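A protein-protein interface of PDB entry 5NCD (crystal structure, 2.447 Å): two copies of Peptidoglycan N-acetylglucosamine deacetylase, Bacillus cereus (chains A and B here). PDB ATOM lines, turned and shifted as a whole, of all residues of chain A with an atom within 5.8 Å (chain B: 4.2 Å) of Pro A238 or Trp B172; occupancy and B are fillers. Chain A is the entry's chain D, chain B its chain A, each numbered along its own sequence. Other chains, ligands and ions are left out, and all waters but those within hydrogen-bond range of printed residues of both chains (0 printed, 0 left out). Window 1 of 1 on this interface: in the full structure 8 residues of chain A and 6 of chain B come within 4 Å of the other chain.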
ATOM      1  N   VAL A 162      -3.062  -4.410 -20.041  1.00  0.00           N
ATOM      2  CA  VAL A 162      -2.554  -5.646 -19.440  1.00  0.00           C
ATOM      3  C   VAL A 162      -1.081  -5.863 -19.758  1.00  0.00           C
ATOM      4  O   VAL A 162      -0.676  -5.862 -20.918  1.00  0.00           O
ATOM      5  CB  VAL A 162      -3.323  -6.872 -19.910  1.00  0.00           C
ATOM      6  CG1 VAL A 162      -2.537  -8.142 -19.599  1.00  0.00           C
ATOM      7  CG2 VAL A 162      -4.716  -6.918 -19.292  1.00  0.00           C
ATOM      8  N   TRP A 163      -0.277  -6.032 -18.719  1.00  0.00           N
ATOM      9  CA  TRP A 163       1.098  -6.450 -18.908  1.00  0.00           C
ATOM     10  C   TRP A 163       1.418  -7.822 -18.291  1.00  0.00           C
ATOM     11  O   TRP A 163       1.148  -8.078 -17.113  1.00  0.00           O
ATOM     12  CB  TRP A 163       2.039  -5.388 -18.360  1.00  0.00           C
ATOM     13  CG  TRP A 163       2.526  -4.478 -19.404  1.00  0.00           C
ATOM     14  CD1 TRP A 163       1.931  -4.234 -20.610  1.00  0.00           C
ATOM     15  CD2 TRP A 163       3.738  -3.697 -19.381  1.00  0.00           C
ATOM     16  NE1 TRP A 163       2.694  -3.342 -21.334  1.00  0.00           N
ATOM     17  CE2 TRP A 163       3.810  -3.003 -20.606  1.00  0.00           C
ATOM     18  CE3 TRP A 163       4.767  -3.512 -18.439  1.00  0.00           C
ATOM     19  CZ2 TRP A 163       4.861  -2.146 -20.926  1.00  0.00           C
ATOM     20  CZ3 TRP A 163       5.836  -2.653 -18.766  1.00  0.00           C
ATOM     21  CH2 TRP A 163       5.865  -1.983 -20.001  1.00  0.00           C
ATOM     22  N   HIS A 236       2.513   3.888 -23.319  1.00  0.00           N
ATOM     23  CA  HIS A 236       2.175   2.465 -23.349  1.00  0.00           C
ATOM     24  C   HIS A 236       2.581   1.763 -24.643  1.00  0.00           C
ATOM     25  O   HIS A 236       2.299   2.260 -25.730  1.00  0.00           O
ATOM     26  CB  HIS A 236       0.672   2.234 -23.159  1.00  0.00           C
ATOM     27  CG  HIS A 236       0.295   0.787 -23.234  1.00  0.00           C
ATOM     28  ND1 HIS A 236       0.493  -0.084 -22.187  1.00  0.00           N
ATOM     29  CD2 HIS A 236      -0.163   0.034 -24.264  1.00  0.00           C
ATOM     30  CE1 HIS A 236       0.123  -1.301 -22.548  1.00  0.00           C
ATOM     31  NE2 HIS A 236      -0.277  -1.257 -23.806  1.00  0.00           N
ATOM     32  N   PHE A 237       3.228   0.606 -24.513  1.00  0.00           N
ATOM     33  CA  PHE A 237       3.449  -0.296 -25.628  1.00  0.00           C
ATOM     34  C   PHE A 237       3.029  -1.708 -25.203  1.00  0.00           C
ATOM     35  O   PHE A 237       3.125  -2.063 -24.045  1.00  0.00           O
ATOM     36  CB  PHE A 237       4.908  -0.256 -26.104  1.00  0.00           C
ATOM     37  CG  PHE A 237       5.893  -0.738 -25.097  1.00  0.00           C
ATOM     38  CD1 PHE A 237       6.440  -2.005 -25.202  1.00  0.00           C
ATOM     39  CD2 PHE A 237       6.292   0.073 -24.046  1.00  0.00           C
ATOM     40  CE1 PHE A 237       7.366  -2.464 -24.272  1.00  0.00           C
ATOM     41  CE2 PHE A 237       7.224  -0.377 -23.097  1.00  0.00           C
ATOM     42  CZ  PHE A 237       7.759  -1.645 -23.206  1.00  0.00           C
ATOM     43  N   PRO A 238       2.546  -2.527 -26.144  1.00  0.00           N
ATOM     44  CA  PRO A 238       1.945  -3.780 -25.684  1.00  0.00           C
ATOM     45  C   PRO A 238       2.983  -4.802 -25.245  1.00  0.00           C
ATOM     46  O   PRO A 238       4.026  -4.909 -25.880  1.00  0.00           O
ATOM     47  CB  PRO A 238       1.183  -4.257 -26.912  1.00  0.00           C
ATOM     48  CG  PRO A 238       1.971  -3.720 -28.041  1.00  0.00           C
ATOM     49  CD  PRO A 238       2.546  -2.418 -27.613  1.00  0.00           C
ATOM     50  N   VAL A 239       2.716  -5.496 -24.143  1.00  0.00           N
ATOM     51  CA  VAL A 239       3.548  -6.611 -23.670  1.00  0.00           C
ATOM     52  C   VAL A 239       2.633  -7.647 -23.019  1.00  0.00           C
ATOM     53  O   VAL A 239       2.276  -7.533 -21.841  1.00  0.00           O
ATOM     54  CB  VAL A 239       4.663  -6.169 -22.661  1.00  0.00           C
ATOM     55  CG1 VAL A 239       5.286  -7.374 -21.942  1.00  0.00           C
ATOM     56  CG2 VAL A 239       5.762  -5.398 -23.357  1.00  0.00           C
ATOM     57  N   ASN A 240       2.229  -8.640 -23.801  1.00  0.00           N
ATOM     58  CA  ASN A 240       1.410  -9.731 -23.292  1.00  0.00           C
ATOM     59  C   ASN A 240       1.538 -11.012 -24.137  1.00  0.00           C
ATOM     60  O   ASN A 240       1.976 -10.988 -25.287  1.00  0.00           O
ATOM     61  CB  ASN A 240      -0.057  -9.304 -23.192  1.00  0.00           C
ATOM     62  CG  ASN A 240      -0.655  -8.906 -24.539  1.00  0.00           C
ATOM     63  OD1 ASN A 240      -1.319  -9.709 -25.200  1.00  0.00           O
ATOM     64  ND2 ASN A 240      -0.463  -7.645 -24.925  1.00  0.00           N
ATOM     65  N   HIS A 243      -0.331 -11.581 -27.570  1.00  0.00           N
ATOM     66  CA  HIS A 243       0.044 -10.700 -28.676  1.00  0.00           C
ATOM     67  C   HIS A 243      -1.133  -9.796 -29.068  1.00  0.00           C
ATOM     68  O   HIS A 243      -1.346  -9.517 -30.248  1.00  0.00           O
ATOM     69  CB  HIS A 243       0.501 -11.501 -29.914  1.00  0.00           C
ATOM     70  CG  HIS A 243       1.452 -12.621 -29.615  1.00  0.00           C
ATOM     71  ND1 HIS A 243       2.359 -12.579 -28.577  1.00  0.00           N
ATOM     72  CD2 HIS A 243       1.625 -13.820 -30.218  1.00  0.00           C
ATOM     73  CE1 HIS A 243       3.054 -13.703 -28.558  1.00  0.00           C
ATOM     74  NE2 HIS A 243       2.627 -14.474 -29.541  1.00  0.00           N
ATOM     75  N   ASP A 244      -1.910  -9.366 -28.085  1.00  0.00           N
ATOM     76  CA  ASP A 244      -3.076  -8.534 -28.342  1.00  0.00           C
ATOM     77  C   ASP A 244      -2.689  -7.079 -28.127  1.00  0.00           C
ATOM     78  O   ASP A 244      -2.521  -6.641 -26.982  1.00  0.00           O
ATOM     79  CB  ASP A 244      -4.242  -8.951 -27.435  1.00  0.00           C
ATOM     80  CG  ASP A 244      -5.546  -8.234 -27.773  1.00  0.00           C
ATOM     81  OD1 ASP A 244      -5.512  -7.187 -28.461  1.00  0.00           O
ATOM     82  OD2 ASP A 244      -6.619  -8.725 -27.353  1.00  0.00           O
ATOM     83  N   ASN A 245      -2.540  -6.321 -29.210  1.00  0.00           N
ATOM     84  CA  ASN A 245      -1.985  -4.973 -29.071  1.00  0.00           C
ATOM     85  C   ASN A 245      -3.040  -3.904 -28.761  1.00  0.00           C
ATOM     86  O   ASN A 245      -2.805  -2.707 -28.935  1.00  0.00           O
ATOM     87  CB  ASN A 245      -1.187  -4.591 -30.317  1.00  0.00           C
ATOM     88  CG  ASN A 245      -2.061  -4.329 -31.526  1.00  0.00           C
ATOM     89  OD1 ASN A 245      -3.222  -4.744 -31.595  1.00  0.00           O
ATOM     90  ND2 ASN A 245      -1.498  -3.621 -32.494  1.00  0.00           N
ATOM     91  N   ARG A 246      -4.198  -4.359 -28.298  1.00  0.00           N
ATOM     92  CA  ARG A 246      -5.220  -3.480 -27.765  1.00  0.00           C
ATOM     93  C   ARG A 246      -4.990  -3.314 -26.260  1.00  0.00           C
ATOM     94  O   ARG A 246      -5.489  -2.374 -25.637  1.00  0.00           O
ATOM     95  CB  ARG A 246      -6.617  -4.038 -28.033  1.00  0.00           C
ATOM     96  CG  ARG A 246      -6.948  -4.310 -29.502  1.00  0.00           C
ATOM     97  CD  ARG A 246      -8.311  -4.968 -29.594  1.00  0.00           C
ATOM     98  NE  ARG A 246      -8.389  -6.120 -28.695  1.00  0.00           N
ATOM     99  CZ  ARG A 246      -9.525  -6.681 -28.295  1.00  0.00           C
ATOM    100  NH1 ARG A 246     -10.682  -6.190 -28.713  1.00  0.00           N
ATOM    101  NH2 ARG A 246      -9.509  -7.722 -27.475  1.00  0.00           N
ATOM    102  N   MET A 247      -4.236  -4.251 -25.686  1.00  0.00           N
ATOM    103  CA  MET A 247      -3.845  -4.192 -24.281  1.00  0.00           C
ATOM    104  C   MET A 247      -2.420  -3.670 -24.127  1.00  0.00           C
ATOM    105  O   MET A 247      -1.831  -3.777 -23.060  1.00  0.00           O
ATOM    106  CB  MET A 247      -3.952  -5.569 -23.626  1.00  0.00           C
ATOM    107  CG  MET A 247      -5.218  -6.323 -23.940  1.00  0.00           C
ATOM    108  SD  MET A 247      -5.278  -7.845 -22.987  1.00  0.00           S
ATOM    109  CE  MET A 247      -3.614  -8.433 -23.213  1.00  0.00           C
ATOM    110  OXT MET A 247      -1.808  -3.148 -25.057  1.00  0.00           O
ATOM    111  N   LEU B 170       8.504  -8.830 -33.502  1.00  0.00           N
ATOM    112  CA  LEU B 170       7.535  -8.012 -32.773  1.00  0.00           C
ATOM    113  C   LEU B 170       6.457  -7.503 -33.723  1.00  0.00           C
ATOM    114  O   LEU B 170       5.872  -6.446 -33.500  1.00  0.00           O
ATOM    115  CB  LEU B 170       8.229  -6.830 -32.055  1.00  0.00           C
ATOM    116  CG  LEU B 170       9.240  -7.139 -30.933  1.00  0.00           C
ATOM    117  CD1 LEU B 170       9.885  -5.869 -30.442  1.00  0.00           C
ATOM    118  CD2 LEU B 170       8.593  -7.880 -29.776  1.00  0.00           C
ATOM    119  N   ASP B 171       6.182  -8.266 -34.774  1.00  0.00           N
ATOM    120  CA  ASP B 171       5.318  -7.786 -35.850  1.00  0.00           C
ATOM    121  C   ASP B 171       3.863  -7.596 -35.410  1.00  0.00           C
ATOM    122  O   ASP B 171       3.128  -6.798 -35.997  1.00  0.00           O
ATOM    123  CB  ASP B 171       5.387  -8.736 -37.059  1.00  0.00           C
ATOM    124  CG  ASP B 171       5.077 -10.186 -36.703  1.00  0.00           C
ATOM    125  OD1 ASP B 171       5.152 -10.560 -35.512  1.00  0.00           O
ATOM    126  OD2 ASP B 171       4.760 -10.960 -37.629  1.00  0.00           O
ATOM    127  N   TRP B 172       3.459  -8.318 -34.371  1.00  0.00           N
ATOM    128  CA  TRP B 172       2.078  -8.320 -33.899  1.00  0.00           C
ATOM    129  C   TRP B 172       1.679  -7.003 -33.222  1.00  0.00           C
ATOM    130  O   TRP B 172       0.487  -6.739 -32.993  1.00  0.00           O
ATOM    131  CB  TRP B 172       1.875  -9.479 -32.920  1.00  0.00           C
ATOM    132  CG  TRP B 172       2.745  -9.335 -31.694  1.00  0.00           C
ATOM    133  CD1 TRP B 172       3.989  -9.848 -31.515  1.00  0.00           C
ATOM    134  CD2 TRP B 172       2.450  -8.582 -30.514  1.00  0.00           C
ATOM    135  NE1 TRP B 172       4.481  -9.483 -30.295  1.00  0.00           N
ATOM    136  CE2 TRP B 172       3.553  -8.711 -29.654  1.00  0.00           C
ATOM    137  CE3 TRP B 172       1.358  -7.819 -30.098  1.00  0.00           C
ATOM    138  CZ2 TRP B 172       3.599  -8.107 -28.397  1.00  0.00           C
ATOM    139  CZ3 TRP B 172       1.401  -7.226 -28.855  1.00  0.00           C
ATOM    140  CH2 TRP B 172       2.517  -7.373 -28.016  1.00  0.00           C
ATOM    141  N   ARG B 173       2.682  -6.200 -32.871  1.00  0.00           N
ATOM    142  CA  ARG B 173       2.449  -4.927 -32.194  1.00  0.00           C
ATOM    143  C   ARG B 173       1.724  -3.976 -33.109  1.00  0.00           C
ATOM    144  O   ARG B 173       0.889  -3.196 -32.674  1.00  0.00           O
ATOM    145  CB  ARG B 173       3.774  -4.307 -31.723  1.00  0.00           C
ATOM    146  CG  ARG B 173       4.490  -5.162 -30.681  1.00  0.00           C
ATOM    147  CD  ARG B 173       5.632  -4.443 -29.973  1.00  0.00           C
ATOM    148  NE  ARG B 173       5.992  -5.171 -28.756  1.00  0.00           N
ATOM    149  CZ  ARG B 173       6.791  -4.716 -27.790  1.00  0.00           C
ATOM    150  NH1 ARG B 173       7.349  -3.518 -27.890  1.00  0.00           N
ATOM    151  NH2 ARG B 173       7.033  -5.469 -26.717  1.00  0.00           N
ATOM    152  N   TYR B 174       2.029  -4.073 -34.394  1.00  0.00           N
ATOM    153  CA  TYR B 174       1.613  -3.070 -35.364  1.00  0.00           C
ATOM    154  C   TYR B 174       0.353  -3.456 -36.138  1.00  0.00           C
ATOM    155  O   TYR B 174       0.015  -2.833 -37.159  1.00  0.00           O
ATOM    156  CB  TYR B 174       2.775  -2.812 -36.313  1.00  0.00           C
ATOM    157  CG  TYR B 174       4.074  -2.720 -35.560  1.00  0.00           C
ATOM    158  CD1 TYR B 174       4.906  -3.824 -35.416  1.00  0.00           C
ATOM    159  CD2 TYR B 174       4.448  -1.537 -34.955  1.00  0.00           C
ATOM    160  CE1 TYR B 174       6.086  -3.731 -34.706  1.00  0.00           C
ATOM    161  CE2 TYR B 174       5.615  -1.433 -34.248  1.00  0.00           C
ATOM    162  CZ  TYR B 174       6.431  -2.522 -34.117  1.00  0.00           C
ATOM    163  OH  TYR B 174       7.597  -2.381 -33.396  1.00  0.00           O
ATOM    164  N   ASN B 175      -0.343  -4.475 -35.636  1.00  0.00           N
ATOM    165  CA  ASN B 175      -1.571  -4.945 -36.266  1.00  0.00           C
ATOM    166  C   ASN B 175      -2.633  -3.845 -36.321  1.00  0.00           C
ATOM    167  O   ASN B 175      -2.752  -3.036 -35.400  1.00  0.00           O
ATOM    168  CB  ASN B 175      -2.109  -6.189 -35.545  1.00  0.00           C
ATOM    169  CG  ASN B 175      -1.181  -7.403 -35.692  1.00  0.00           C
ATOM    170  OD1 ASN B 175      -0.299  -7.424 -36.552  1.00  0.00           O
ATOM    171  ND2 ASN B 175      -1.383  -8.416 -34.851  1.00  0.00           N
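The guanidinium group of Arg B173 is in hydrogen-bond range of the backbone carbonyl oxygen of Pro A238 (3.2 Å). ND2 of Asn A245 lies within hydrogen-bond range of O of Arg B173. O of Asn B175 lies within hydrogen-bond range of ND2 of Asn A245 (3.2 Å).
The side-chain amide nitrogen (ND2) of Asn B175 is in hydrogen-bond range of the backbone carbonyl oxygen (O) of Trp B172, at 3.1 Å. O of Phe A237 sits at hydrogen-bond distance from NE1 of Trp A163 (3.0 Å). OD1 of Asn A240 lies within hydrogen-bond range of N of His A243.
Phe A237 touches Arg B173 (CD1 to NH1, 3.2 Å). Trp B172 touches Pro A238 (CZ3 to CB, 3.6 Å). CG2 of Val A239 touches NH2 of Arg B173 (3.6 Å). O of His A243 touches CE3 of Trp B172 (3.2 Å). Asn A245 touches Trp B172.
Of chain B, only Trp B172 (3.6 Å) and Arg B173 (3.2 Å) come within 4 Å of Pro A238. Of the printed residues of chain B, Val A239 touches Arg B173 (3.6 Å). Of the printed residues of chain B, His A243 touches Trp B172. Asp A244 touches none of the printed residues of chain B. Printed residues of chain B within 4 Å of Asn A245: Trp B172, Arg B173 and Asn B175. Printed residues of chain A within 4 Å of Trp B172: Pro A238 (3.6 Å), His A243 (3.2 Å) and Asn A245 (3.7 Å). Of the printed residues of chain A, Arg B173 touches Phe A237 (3.2 Å), Pro A238 (3.2 Å), Val A239 (3.6 Å) and Asn A245 (2.4 Å). The nearest printed residue of chain A that does not touch Trp B172 is Asp A244 (4.02 Å).
Of the 6 printed residues of chain B, 3 touch a printed residue of chain A. Hydrophobic or aromatic side chains of chain B within 4 Å of the printed part of chain A: Trp B172. Hydrophobic or aromatic side chains of chain A within 4 Å of the printed part of chain B: Phe A237, Pro A238, Val A239 and His A243.
No position is printed for both chains. Of the 8 pairs that touch across the chains among the printed residues, none has its exchanged pair printed and touching as well.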
